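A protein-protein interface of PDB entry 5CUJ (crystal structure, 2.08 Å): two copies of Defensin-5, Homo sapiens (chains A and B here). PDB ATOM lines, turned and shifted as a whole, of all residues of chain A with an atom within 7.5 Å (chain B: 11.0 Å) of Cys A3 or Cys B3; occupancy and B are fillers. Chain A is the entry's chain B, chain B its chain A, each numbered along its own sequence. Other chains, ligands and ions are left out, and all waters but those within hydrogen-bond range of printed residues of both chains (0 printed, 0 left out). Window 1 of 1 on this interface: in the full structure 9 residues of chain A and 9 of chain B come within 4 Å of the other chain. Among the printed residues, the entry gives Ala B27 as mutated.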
ATOM      1  N   ALA A   1     -13.768 -22.173  27.610  1.00  0.00           N
ATOM      2  CA  ALA A   1     -12.498 -21.431  27.327  1.00  0.00           C
ATOM      3  C   ALA A   1     -12.754 -19.946  27.107  1.00  0.00           C
ATOM      4  O   ALA A   1     -13.899 -19.519  26.987  1.00  0.00           O
ATOM      5  CB  ALA A   1     -11.795 -22.020  26.111  1.00  0.00           C
ATOM      6  N   THR A   2     -11.676 -19.170  27.070  1.00  0.00           N
ATOM      7  CA  THR A   2     -11.740 -17.761  26.712  1.00  0.00           C
ATOM      8  C   THR A   2     -11.264 -17.635  25.276  1.00  0.00           C
ATOM      9  O   THR A   2     -10.120 -17.963  24.973  1.00  0.00           O
ATOM     10  CB  THR A   2     -10.861 -16.906  27.634  1.00  0.00           C
ATOM     11  OG1 THR A   2     -11.307 -17.065  28.986  1.00  0.00           O
ATOM     12  CG2 THR A   2     -10.932 -15.425  27.238  1.00  0.00           C
ATOM     13  N   CYS A   3     -12.149 -17.175  24.393  1.00  0.00           N
ATOM     14  CA  CYS A   3     -11.861 -17.107  22.961  1.00  0.00           C
ATOM     15  C   CYS A   3     -12.234 -15.762  22.368  1.00  0.00           C
ATOM     16  O   CYS A   3     -13.061 -15.040  22.924  1.00  0.00           O
ATOM     17  CB  CYS A   3     -12.631 -18.189  22.209  1.00  0.00           C
ATOM     18  SG  CYS A   3     -12.417 -19.867  22.826  1.00  0.00           S
ATOM     19  N   TYR A   4     -11.621 -15.448  21.228  1.00  0.00           N
ATOM     20  CA  TYR A   4     -11.899 -14.216  20.487  1.00  0.00           C
ATOM     21  C   TYR A   4     -12.006 -14.507  18.993  1.00  0.00           C
ATOM     22  O   TYR A   4     -11.324 -15.395  18.467  1.00  0.00           O
ATOM     23  CB  TYR A   4     -10.798 -13.181  20.733  1.00  0.00           C
ATOM     24  CG  TYR A   4     -10.526 -12.935  22.199  1.00  0.00           C
ATOM     25  CD1 TYR A   4      -9.452 -13.552  22.844  1.00  0.00           C
ATOM     26  CD2 TYR A   4     -11.359 -12.111  22.951  1.00  0.00           C
ATOM     27  CE1 TYR A   4      -9.208 -13.340  24.195  1.00  0.00           C
ATOM     28  CE2 TYR A   4     -11.124 -11.891  24.300  1.00  0.00           C
ATOM     29  CZ  TYR A   4     -10.050 -12.508  24.919  1.00  0.00           C
ATOM     30  OH  TYR A   4      -9.822 -12.287  26.257  1.00  0.00           O
ATOM     31  N   CYS A   5     -12.882 -13.766  18.321  1.00  0.00           N
ATOM     32  CA  CYS A   5     -12.979 -13.816  16.873  1.00  0.00           C
ATOM     33  C   CYS A   5     -12.015 -12.768  16.336  1.00  0.00           C
ATOM     34  O   CYS A   5     -12.185 -11.576  16.603  1.00  0.00           O
ATOM     35  CB  CYS A   5     -14.410 -13.539  16.418  1.00  0.00           C
ATOM     36  SG  CYS A   5     -14.719 -14.060  14.723  1.00  0.00           S
ATOM     37  N   ARG A   6     -10.999 -13.214  15.598  1.00  0.00           N
ATOM     38  CA  ARG A   6      -9.852 -12.368  15.277  1.00  0.00           C
ATOM     39  C   ARG A   6      -9.730 -12.035  13.792  1.00  0.00           C
ATOM     40  O   ARG A   6     -10.044 -12.864  12.935  1.00  0.00           O
ATOM     41  CB  ARG A   6      -8.562 -13.030  15.763  1.00  0.00           C
ATOM     42  CG  ARG A   6      -8.460 -13.139  17.279  1.00  0.00           C
ATOM     43  CD  ARG A   6      -7.017 -13.044  17.745  1.00  0.00           C
ATOM     44  NE  ARG A   6      -6.906 -12.980  19.201  1.00  0.00           N
ATOM     45  CZ  ARG A   6      -7.095 -11.886  19.943  1.00  0.00           C
ATOM     46  NH1 ARG A   6      -7.452 -10.721  19.396  1.00  0.00           N
ATOM     47  NH2 ARG A   6      -6.947 -11.960  21.260  1.00  0.00           N
ATOM     48  N   GLU A  14      -2.433 -18.193  22.210  1.00  0.00           N
ATOM     49  CA  GLU A  14      -3.713 -18.641  21.670  1.00  0.00           C
ATOM     50  C   GLU A  14      -3.507 -19.693  20.585  1.00  0.00           C
ATOM     51  O   GLU A  14      -2.429 -19.791  19.993  1.00  0.00           O
ATOM     52  CB  GLU A  14      -4.471 -17.454  21.074  1.00  0.00           C
ATOM     53  CG  GLU A  14      -4.907 -16.411  22.090  1.00  0.00           C
ATOM     54  CD  GLU A  14      -5.601 -15.209  21.466  1.00  0.00           C
ATOM     55  OE1 GLU A  14      -5.582 -15.060  20.227  1.00  0.00           O
ATOM     56  OE2 GLU A  14      -6.176 -14.398  22.219  1.00  0.00           O
ATOM     57  N   SER A  15      -4.558 -20.468  20.333  1.00  0.00           N
ATOM     58  CA  SER A  15      -4.564 -21.480  19.281  1.00  0.00           C
ATOM     59  C   SER A  15      -5.825 -21.345  18.429  1.00  0.00           C
ATOM     60  O   SER A  15      -6.923 -21.145  18.960  1.00  0.00           O
ATOM     61  CB  SER A  15      -4.496 -22.879  19.896  1.00  0.00           C
ATOM     62  OG  SER A  15      -3.280 -23.077  20.599  1.00  0.00           O
ATOM     63  N   SER A  17      -8.863 -22.421  17.049  1.00  0.00           N
ATOM     64  CA  SER A  17      -9.724 -23.476  17.586  1.00  0.00           C
ATOM     65  C   SER A  17     -11.088 -23.606  16.895  1.00  0.00           C
ATOM     66  O   SER A  17     -11.935 -24.372  17.357  1.00  0.00           O
ATOM     67  CB  SER A  17      -9.927 -23.237  19.082  1.00  0.00           C
ATOM     68  OG  SER A  17      -8.684 -23.050  19.734  1.00  0.00           O
ATOM     69  N   LEU A  29     -11.148 -18.246  14.951  1.00  0.00           N
ATOM     70  CA  LEU A  29     -11.503 -18.330  16.362  1.00  0.00           C
ATOM     71  C   LEU A  29     -10.254 -18.716  17.133  1.00  0.00           C
ATOM     72  O   LEU A  29      -9.740 -19.830  16.973  1.00  0.00           O
ATOM     73  CB  LEU A  29     -12.586 -19.363  16.625  1.00  0.00           C
ATOM     74  CG  LEU A  29     -12.884 -19.495  18.130  1.00  0.00           C
ATOM     75  CD1 LEU A  29     -13.760 -18.343  18.602  1.00  0.00           C
ATOM     76  CD2 LEU A  29     -13.499 -20.850  18.447  1.00  0.00           C
ATOM     77  N   CYS A  30      -9.798 -17.810  17.995  1.00  0.00           N
ATOM     78  CA  CYS A  30      -8.578 -18.001  18.770  1.00  0.00           C
ATOM     79  C   CYS A  30      -8.932 -18.149  20.246  1.00  0.00           C
ATOM     80  O   CYS A  30      -9.587 -17.281  20.816  1.00  0.00           O
ATOM     81  CB  CYS A  30      -7.638 -16.819  18.557  1.00  0.00           C
ATOM     82  SG  CYS A  30      -7.165 -16.578  16.829  1.00  0.00           S
ATOM     83  N   CYS A  31      -8.490 -19.248  20.856  1.00  0.00           N
ATOM     84  CA  CYS A  31      -8.843 -19.568  22.236  1.00  0.00           C
ATOM     85  C   CYS A  31      -7.626 -19.726  23.136  1.00  0.00           C
ATOM     86  O   CYS A  31      -6.609 -20.300  22.734  1.00  0.00           O
ATOM     87  CB  CYS A  31      -9.660 -20.851  22.276  1.00  0.00           C
ATOM     88  SG  CYS A  31     -11.233 -20.703  21.415  1.00  0.00           S
ATOM     89  N   ARG A  32      -7.756 -19.213  24.359  1.00  0.00           N
ATOM     90  CA  ARG A  32      -6.784 -19.435  25.420  1.00  0.00           C
ATOM     91  C   ARG A  32      -7.285 -20.538  26.338  1.00  0.00           C
ATOM     92  O   ARG A  32      -6.477 -21.243  26.896  1.00  0.00           O
ATOM     93  CB  ARG A  32      -6.555 -18.158  26.228  1.00  0.00           C
ATOM     94  CG  ARG A  32      -5.916 -17.039  25.426  1.00  0.00           C
ATOM     95  CD  ARG A  32      -5.461 -15.878  26.299  1.00  0.00           C
ATOM     96  NE  ARG A  32      -6.587 -15.164  26.910  1.00  0.00           N
ATOM     97  CZ  ARG A  32      -7.039 -15.317  28.160  1.00  0.00           C
ATOM     98  NH1 ARG A  32      -6.479 -16.172  29.021  1.00  0.00           N
ATOM     99  NH2 ARG A  32      -8.078 -14.589  28.561  1.00  0.00           N
ATOM    100  OXT ARG A  32      -8.477 -20.760  26.551  1.00  0.00           O
ATOM    101  N   ALA B   1     -14.477 -13.298  24.699  1.00  0.00           N
ATOM    102  CA  ALA B   1     -15.717 -13.970  25.202  1.00  0.00           C
ATOM    103  C   ALA B   1     -15.399 -15.317  25.836  1.00  0.00           C
ATOM    104  O   ALA B   1     -14.284 -15.819  25.707  1.00  0.00           O
ATOM    105  CB  ALA B   1     -16.719 -14.151  24.072  1.00  0.00           C
ATOM    106  N   THR B   2     -16.386 -15.889  26.525  1.00  0.00           N
ATOM    107  CA  THR B   2     -16.273 -17.235  27.095  1.00  0.00           C
ATOM    108  C   THR B   2     -17.016 -18.208  26.180  1.00  0.00           C
ATOM    109  O   THR B   2     -18.231 -18.100  26.036  1.00  0.00           O
ATOM    110  CB  THR B   2     -16.864 -17.298  28.519  1.00  0.00           C
ATOM    111  OG1 THR B   2     -16.219 -16.325  29.352  1.00  0.00           O
ATOM    112  CG2 THR B   2     -16.681 -18.690  29.134  1.00  0.00           C
ATOM    113  N   CYS B   3     -16.285 -19.149  25.573  1.00  0.00           N
ATOM    114  CA  CYS B   3     -16.842 -20.047  24.552  1.00  0.00           C
ATOM    115  C   CYS B   3     -16.579 -21.525  24.838  1.00  0.00           C
ATOM    116  O   CYS B   3     -15.580 -21.877  25.474  1.00  0.00           O
ATOM    117  CB  CYS B   3     -16.279 -19.707  23.172  1.00  0.00           C
ATOM    118  SG  CYS B   3     -16.534 -17.998  22.650  1.00  0.00           S
ATOM    119  N   TYR B   4     -17.482 -22.379  24.354  1.00  0.00           N
ATOM    120  CA  TYR B   4     -17.359 -23.835  24.505  1.00  0.00           C
ATOM    121  C   TYR B   4     -17.786 -24.543  23.231  1.00  0.00           C
ATOM    122  O   TYR B   4     -18.655 -24.057  22.505  1.00  0.00           O
ATOM    123  CB  TYR B   4     -18.210 -24.328  25.677  1.00  0.00           C
ATOM    124  CG  TYR B   4     -17.831 -23.693  26.987  1.00  0.00           C
ATOM    125  CD1 TYR B   4     -18.516 -22.577  27.467  1.00  0.00           C
ATOM    126  CD2 TYR B   4     -16.763 -24.181  27.736  1.00  0.00           C
ATOM    127  CE1 TYR B   4     -18.160 -21.980  28.667  1.00  0.00           C
ATOM    128  CE2 TYR B   4     -16.397 -23.591  28.936  1.00  0.00           C
ATOM    129  CZ  TYR B   4     -17.096 -22.490  29.397  1.00  0.00           C
ATOM    130  OH  TYR B   4     -16.734 -21.904  30.588  1.00  0.00           O
ATOM    131  N   CYS B   5     -17.164 -25.687  22.962  1.00  0.00           N
ATOM    132  CA  CYS B   5     -17.527 -26.512  21.820  1.00  0.00           C
ATOM    133  C   CYS B   5     -18.578 -27.516  22.278  1.00  0.00           C
ATOM    134  O   CYS B   5     -18.269 -28.435  23.037  1.00  0.00           O
ATOM    135  CB  CYS B   5     -16.293 -27.214  21.251  1.00  0.00           C
ATOM    136  SG  CYS B   5     -16.476 -27.753  19.537  1.00  0.00           S
ATOM    137  N   ARG B   6     -19.817 -27.335  21.822  1.00  0.00           N
ATOM    138  CA  ARG B   6     -20.956 -28.065  22.375  1.00  0.00           C
ATOM    139  C   ARG B   6     -21.554 -29.120  21.444  1.00  0.00           C
ATOM    140  O   ARG B   6     -21.655 -28.914  20.233  1.00  0.00           O
ATOM    141  CB  ARG B   6     -22.046 -27.087  22.805  1.00  0.00           C
ATOM    142  CG  ARG B   6     -21.607 -26.148  23.914  1.00  0.00           C
ATOM    143  CD  ARG B   6     -22.740 -25.854  24.885  1.00  0.00           C
ATOM    144  NE  ARG B   6     -22.278 -25.052  26.013  1.00  0.00           N
ATOM    145  CZ  ARG B   6     -21.571 -25.518  27.044  1.00  0.00           C
ATOM    146  NH1 ARG B   6     -21.210 -26.801  27.118  1.00  0.00           N
ATOM    147  NH2 ARG B   6     -21.211 -24.684  28.017  1.00  0.00           N
ATOM    148  N   THR B   7     -21.942 -30.248  22.044  1.00  0.00           N
ATOM    149  CA  THR B   7     -22.674 -31.316  21.364  1.00  0.00           C
ATOM    150  C   THR B   7     -24.177 -31.066  21.426  1.00  0.00           C
ATOM    151  O   THR B   7     -24.896 -31.385  20.480  1.00  0.00           O
ATOM    152  CB  THR B   7     -22.394 -32.686  22.008  1.00  0.00           C
ATOM    153  OG1 THR B   7     -22.708 -32.638  23.406  1.00  0.00           O
ATOM    154  CG2 THR B   7     -20.938 -33.070  21.831  1.00  0.00           C
ATOM    155  N   CYS B  10     -26.800 -24.663  22.949  1.00  0.00           N
ATOM    156  CA  CYS B  10     -26.099 -23.681  23.777  1.00  0.00           C
ATOM    157  C   CYS B  10     -26.904 -23.426  25.048  1.00  0.00           C
ATOM    158  O   CYS B  10     -28.134 -23.482  25.025  1.00  0.00           O
ATOM    159  CB  CYS B  10     -25.895 -22.364  23.015  1.00  0.00           C
ATOM    160  SG  CYS B  10     -24.898 -22.467  21.503  1.00  0.00           S
ATOM    161  N   ALA B  11     -26.212 -23.169  26.155  1.00  0.00           N
ATOM    162  CA  ALA B  11     -26.880 -22.752  27.392  1.00  0.00           C
ATOM    163  C   ALA B  11     -27.652 -21.458  27.121  1.00  0.00           C
ATOM    164  O   ALA B  11     -27.273 -20.695  26.234  1.00  0.00           O
ATOM    165  CB  ALA B  11     -25.864 -22.553  28.509  1.00  0.00           C
ATOM    166  N   ARG B  13     -27.856 -18.711  28.711  1.00  0.00           N
ATOM    167  CA  ARG B  13     -26.825 -17.663  28.829  1.00  0.00           C
ATOM    168  C   ARG B  13     -25.938 -17.450  27.583  1.00  0.00           C
ATOM    169  O   ARG B  13     -25.400 -16.356  27.389  1.00  0.00           O
ATOM    170  CB  ARG B  13     -25.925 -17.932  30.052  1.00  0.00           C
ATOM    171  CG  ARG B  13     -25.772 -19.402  30.438  1.00  0.00           C
ATOM    172  CD  ARG B  13     -24.486 -19.686  31.180  1.00  0.00           C
ATOM    173  NE  ARG B  13     -23.376 -19.895  30.259  1.00  0.00           N
ATOM    174  CZ  ARG B  13     -22.151 -20.287  30.608  1.00  0.00           C
ATOM    175  NH1 ARG B  13     -21.828 -20.512  31.881  1.00  0.00           N
ATOM    176  NH2 ARG B  13     -21.224 -20.443  29.670  1.00  0.00           N
ATOM    177  N   GLU B  14     -25.773 -18.489  26.765  1.00  0.00           N
ATOM    178  CA  GLU B  14     -24.860 -18.474  25.612  1.00  0.00           C
ATOM    179  C   GLU B  14     -25.576 -18.201  24.298  1.00  0.00           C
ATOM    180  O   GLU B  14     -26.781 -18.405  24.185  1.00  0.00           O
ATOM    181  CB  GLU B  14     -24.150 -19.825  25.483  1.00  0.00           C
ATOM    182  CG  GLU B  14     -23.266 -20.191  26.662  1.00  0.00           C
ATOM    183  CD  GLU B  14     -22.829 -21.648  26.674  1.00  0.00           C
ATOM    184  OE1 GLU B  14     -23.475 -22.495  26.015  1.00  0.00           O
ATOM    185  OE2 GLU B  14     -21.832 -21.955  27.366  1.00  0.00           O
ATOM    186  N   SER B  15     -24.811 -17.773  23.297  1.00  0.00           N
ATOM    187  CA  SER B  15     -25.306 -17.620  21.931  1.00  0.00           C
ATOM    188  C   SER B  15     -24.431 -18.440  20.992  1.00  0.00           C
ATOM    189  O   SER B  15     -23.207 -18.465  21.138  1.00  0.00           O
ATOM    190  CB  SER B  15     -25.276 -16.149  21.508  1.00  0.00           C
ATOM    191  OG  SER B  15     -26.152 -15.367  22.305  1.00  0.00           O
ATOM    192  N   LEU B  16     -25.056 -19.115  20.031  1.00  0.00           N
ATOM    193  CA  LEU B  16     -24.312 -19.827  19.000  1.00  0.00           C
ATOM    194  C   LEU B  16     -23.476 -18.807  18.242  1.00  0.00           C
ATOM    195  O   LEU B  16     -24.017 -17.931  17.587  1.00  0.00           O
ATOM    196  CB  LEU B  16     -25.265 -20.543  18.042  1.00  0.00           C
ATOM    197  CG  LEU B  16     -24.643 -21.241  16.828  1.00  0.00           C
ATOM    198  CD1 LEU B  16     -23.569 -22.230  17.254  1.00  0.00           C
ATOM    199  CD2 LEU B  16     -25.722 -21.937  16.016  1.00  0.00           C
ATOM    200  N   SER B  17     -22.161 -18.904  18.343  1.00  0.00           N
ATOM    201  CA  SER B  17     -21.303 -17.845  17.828  1.00  0.00           C
ATOM    202  C   SER B  17     -20.330 -18.315  16.759  1.00  0.00           C
ATOM    203  O   SER B  17     -19.404 -17.584  16.404  1.00  0.00           O
ATOM    204  CB  SER B  17     -20.546 -17.220  18.989  1.00  0.00           C
ATOM    205  OG  SER B  17     -21.445 -16.842  20.012  1.00  0.00           O
ATOM    206  N   GLY B  18     -20.541 -19.518  16.229  1.00  0.00           N
ATOM    207  CA  GLY B  18     -19.659 -20.063  15.199  1.00  0.00           C
ATOM    208  C   GLY B  18     -19.550 -21.576  15.204  1.00  0.00           C
ATOM    209  O   GLY B  18     -20.401 -22.272  15.768  1.00  0.00           O
ATOM    210  N   VAL B  19     -18.478 -22.073  14.591  1.00  0.00           N
ATOM    211  CA  VAL B  19     -18.288 -23.502  14.360  1.00  0.00           C
ATOM    212  C   VAL B  19     -16.955 -23.958  14.946  1.00  0.00           C
ATOM    213  O   VAL B  19     -15.939 -23.273  14.813  1.00  0.00           O
ATOM    214  CB  VAL B  19     -18.314 -23.830  12.849  1.00  0.00           C
ATOM    215  CG1 VAL B  19     -18.334 -25.339  12.625  1.00  0.00           C
ATOM    216  CG2 VAL B  19     -19.514 -23.171  12.174  1.00  0.00           C
ATOM    217  N   CYS B  20     -16.980 -25.118  15.594  1.00  0.00           N
ATOM    218  CA  CYS B  20     -15.775 -25.796  16.076  1.00  0.00           C
ATOM    219  C   CYS B  20     -15.905 -27.281  15.729  1.00  0.00           C
ATOM    220  O   CYS B  20     -16.817 -27.662  14.988  1.00  0.00           O
ATOM    221  CB  CYS B  20     -15.611 -25.573  17.583  1.00  0.00           C
ATOM    222  SG  CYS B  20     -17.046 -26.058  18.562  1.00  0.00           S
ATOM    223  N   GLU B  21     -15.001 -28.120  16.232  1.00  0.00           N
ATOM    224  CA  GLU B  21     -15.058 -29.550  15.941  1.00  0.00           C
ATOM    225  C   GLU B  21     -14.838 -30.442  17.155  1.00  0.00           C
ATOM    226  O   GLU B  21     -13.932 -30.206  17.956  1.00  0.00           O
ATOM    227  CB  GLU B  21     -14.042 -29.904  14.853  1.00  0.00           C
ATOM    228  CG  GLU B  21     -14.585 -29.750  13.444  1.00  0.00           C
ATOM    229  CD  GLU B  21     -13.633 -30.282  12.396  1.00  0.00           C
ATOM    230  OE1 GLU B  21     -12.406 -30.163  12.591  1.00  0.00           O
ATOM    231  OE2 GLU B  21     -14.111 -30.805  11.366  1.00  0.00           O
ATOM    232  N   ILE B  22     -15.674 -31.477  17.258  1.00  0.00           N
ATOM    233  CA  ILE B  22     -15.523 -32.538  18.248  1.00  0.00           C
ATOM    234  C   ILE B  22     -15.267 -33.838  17.488  1.00  0.00           C
ATOM    235  O   ILE B  22     -16.181 -34.389  16.866  1.00  0.00           O
ATOM    236  CB  ILE B  22     -16.775 -32.657  19.139  1.00  0.00           C
ATOM    237  CG1 ILE B  22     -16.945 -31.368  19.953  1.00  0.00           C
ATOM    238  CG2 ILE B  22     -16.673 -33.873  20.056  1.00  0.00           C
ATOM    239  CD1 ILE B  22     -18.266 -31.242  20.673  1.00  0.00           C
ATOM    240  N   ALA B  27     -19.420 -28.951  15.412  1.00  0.00           N
ATOM    241  CA  ALA B  27     -20.131 -28.724  16.660  1.00  0.00           C
ATOM    242  C   ALA B  27     -20.422 -27.237  16.842  1.00  0.00           C
ATOM    243  O   ALA B  27     -19.760 -26.380  16.246  1.00  0.00           O
ATOM    244  CB  ALA B  27     -19.312 -29.258  17.822  1.00  0.00           C
ATOM    245  N   ARG B  28     -21.421 -26.951  17.671  1.00  0.00           N
ATOM    246  CA  ARG B  28     -21.788 -25.579  18.011  1.00  0.00           C
ATOM    247  C   ARG B  28     -20.649 -24.925  18.782  1.00  0.00           C
ATOM    248  O   ARG B  28     -20.120 -25.523  19.715  1.00  0.00           O
ATOM    249  CB  ARG B  28     -23.032 -25.549  18.909  1.00  0.00           C
ATOM    250  CG  ARG B  28     -24.317 -26.092  18.308  1.00  0.00           C
ATOM    251  CD  ARG B  28     -25.425 -26.033  19.352  1.00  0.00           C
ATOM    252  NE  ARG B  28     -26.705 -26.552  18.867  1.00  0.00           N
ATOM    253  CZ  ARG B  28     -27.043 -27.842  18.776  1.00  0.00           C
ATOM    254  NH1 ARG B  28     -26.196 -28.809  19.130  1.00  0.00           N
ATOM    255  NH2 ARG B  28     -28.249 -28.171  18.317  1.00  0.00           N
ATOM    256  N   LEU B  29     -20.263 -23.717  18.386  1.00  0.00           N
ATOM    257  CA  LEU B  29     -19.469 -22.859  19.253  1.00  0.00           C
ATOM    258  C   LEU B  29     -20.452 -21.968  20.000  1.00  0.00           C
ATOM    259  O   LEU B  29     -21.140 -21.148  19.387  1.00  0.00           O
ATOM    260  CB  LEU B  29     -18.488 -22.004  18.459  1.00  0.00           C
ATOM    261  CG  LEU B  29     -17.593 -21.094  19.308  1.00  0.00           C
ATOM    262  CD1 LEU B  29     -16.578 -21.891  20.122  1.00  0.00           C
ATOM    263  CD2 LEU B  29     -16.897 -20.081  18.413  1.00  0.00           C
ATOM    264  N   CYS B  30     -20.514 -22.128  21.318  1.00  0.00           N
ATOM    265  CA  CYS B  30     -21.447 -21.372  22.149  1.00  0.00           C
ATOM    266  C   CYS B  30     -20.667 -20.413  23.028  1.00  0.00           C
ATOM    267  O   CYS B  30     -19.829 -20.849  23.821  1.00  0.00           O
ATOM    268  CB  CYS B  30     -22.274 -22.318  23.012  1.00  0.00           C
ATOM    269  SG  CYS B  30     -23.234 -23.504  22.050  1.00  0.00           S
ATOM    270  N   CYS B  31     -20.944 -19.117  22.881  1.00  0.00           N
ATOM    271  CA  CYS B  31     -20.213 -18.072  23.596  1.00  0.00           C
ATOM    272  C   CYS B  31     -21.127 -17.193  24.442  1.00  0.00           C
ATOM    273  O   CYS B  31     -22.344 -17.178  24.254  1.00  0.00           O
ATOM    274  CB  CYS B  31     -19.440 -17.190  22.616  1.00  0.00           C
ATOM    275  SG  CYS B  31     -18.257 -18.078  21.582  1.00  0.00           S
ATOM    276  N   ARG B  32     -20.518 -16.465  25.374  1.00  0.00           N
ATOM    277  CA  ARG B  32     -21.220 -15.453  26.163  1.00  0.00           C
ATOM    278  C   ARG B  32     -20.266 -14.339  26.582  1.00  0.00           C
ATOM    279  O   ARG B  32     -20.703 -13.276  27.015  1.00  0.00           O
ATOM    280  CB  ARG B  32     -21.867 -16.085  27.398  1.00  0.00           C
ATOM    281  CG  ARG B  32     -20.876 -16.686  28.388  1.00  0.00           C
ATOM    282  CD  ARG B  32     -21.514 -16.918  29.743  1.00  0.00           C
ATOM    283  NE  ARG B  32     -20.546 -17.415  30.725  1.00  0.00           N
ATOM    284  CZ  ARG B  32     -19.701 -16.653  31.429  1.00  0.00           C
ATOM    285  NH1 ARG B  32     -19.644 -15.328  31.266  1.00  0.00           N
ATOM    286  NH2 ARG B  32     -18.876 -17.233  32.299  1.00  0.00           N
ATOM    287  OXT ARG B  32     -19.043 -14.481  26.514  1.00  0.00           O
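The backbone carbonyl oxygen (O) of Ala B1 lies within hydrogen-bond range of the backbone NH (N) of Cys A3.
The backbone NH (N) of Cys B3 lies within hydrogen-bond range of the backbone carbonyl oxygen (O) of Ala A1.
SG of Cys B5 is disulfide-bonded to SG of Cys B20.
O of Leu B29 is in hydrogen-bond range of N of Ser B17 (2.7 Å).
The backbone NH (N) of Arg A32 sits at hydrogen-bond distance from the backbone carbonyl oxygen (O) of Thr A2 (2.7 Å).
The side-chain sulfur of Cys A31 is disulfide-bonded to the side-chain sulfur of Cys A3, at 2.0 Å.
N of Tyr A4 is in hydrogen-bond range of O of Cys A30 (2.8 Å).
The backbone carbonyl oxygen (O) of Leu A29 lies within hydrogen-bond range of the backbone NH (N) of Ser A17 (2.7 Å).
Ala A1 touches Thr B2, and with the chains exchanged Thr A2 touches Ala B1.
Ala A1 touches Cys B3, and with the chains exchanged Cys A3 touches Ala B1.
Cys B3 touches its own counterpart, Cys A3.
Leu A29 touches its own counterpart, Leu B29.
Positions printed for both chains: 1, 2, 3, 4, 5, 6, 14, 15, 17, 29, 30, 31 and 32.
Of the 10 pairs that touch across the chains among the printed residues, 9 have their exchanged pair printed and touching as well.
Of chain B, only Ala B1 (3.4 Å) comes within 4 Å of Thr A2.
Cys A3 touches just these residues of chain B: Ala B1 and Cys B3.
Tyr A4 touches just one residue of chain B: Ala B1.
Of the printed residues of chain B, Leu A29 touches Leu B29 (3.5 Å).
No residue of chain B comes within 4 Å of Cys A31.
Printed residues of chain A within 4 Å of Ala B1: Ala A1, Thr A2, Cys A3 and Tyr A4.
Cys B3 touches just these residues of chain A: Ala A1 (2.8 Å) and Cys A3 (3.9 Å).
Of the printed residues of chain A, Tyr B4 touches Ala A1.
Ser B17 touches none of the printed residues of chain A.
Of the printed residues of chain A, Cys B20 touches Ser A17.
Of the printed residues of chain A, Leu B29 touches Leu A29.
The nearest residue of chain A that does not touch Cys B3 is Thr A2 (4.8 Å).
Hydrophobic or aromatic side chains of chain B that line the printed part of chain A: Ala B1, Tyr B4 and Leu B29.
Hydrophobic or aromatic side chains of chain A that line the printed part of chain B: Ala A1, Tyr A4 and Leu A29.
Among the printed residues, 10 pairs touch across the chains.
Ala B1 touches Ala A1.
Ala A1 touches Thr B2.
Ala A1 touches Tyr B4.
Ala B1 touches Thr A2.
Cys B3 touches Cys A3 (CB to SG, 3.9 Å).
CE2 of Tyr A4 touches N of Ala B1 (3.7 Å).
Cys B20 touches Ser A17.
Leu A29 touches Leu B29 (CD2 to CD2, 3.5 Å).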
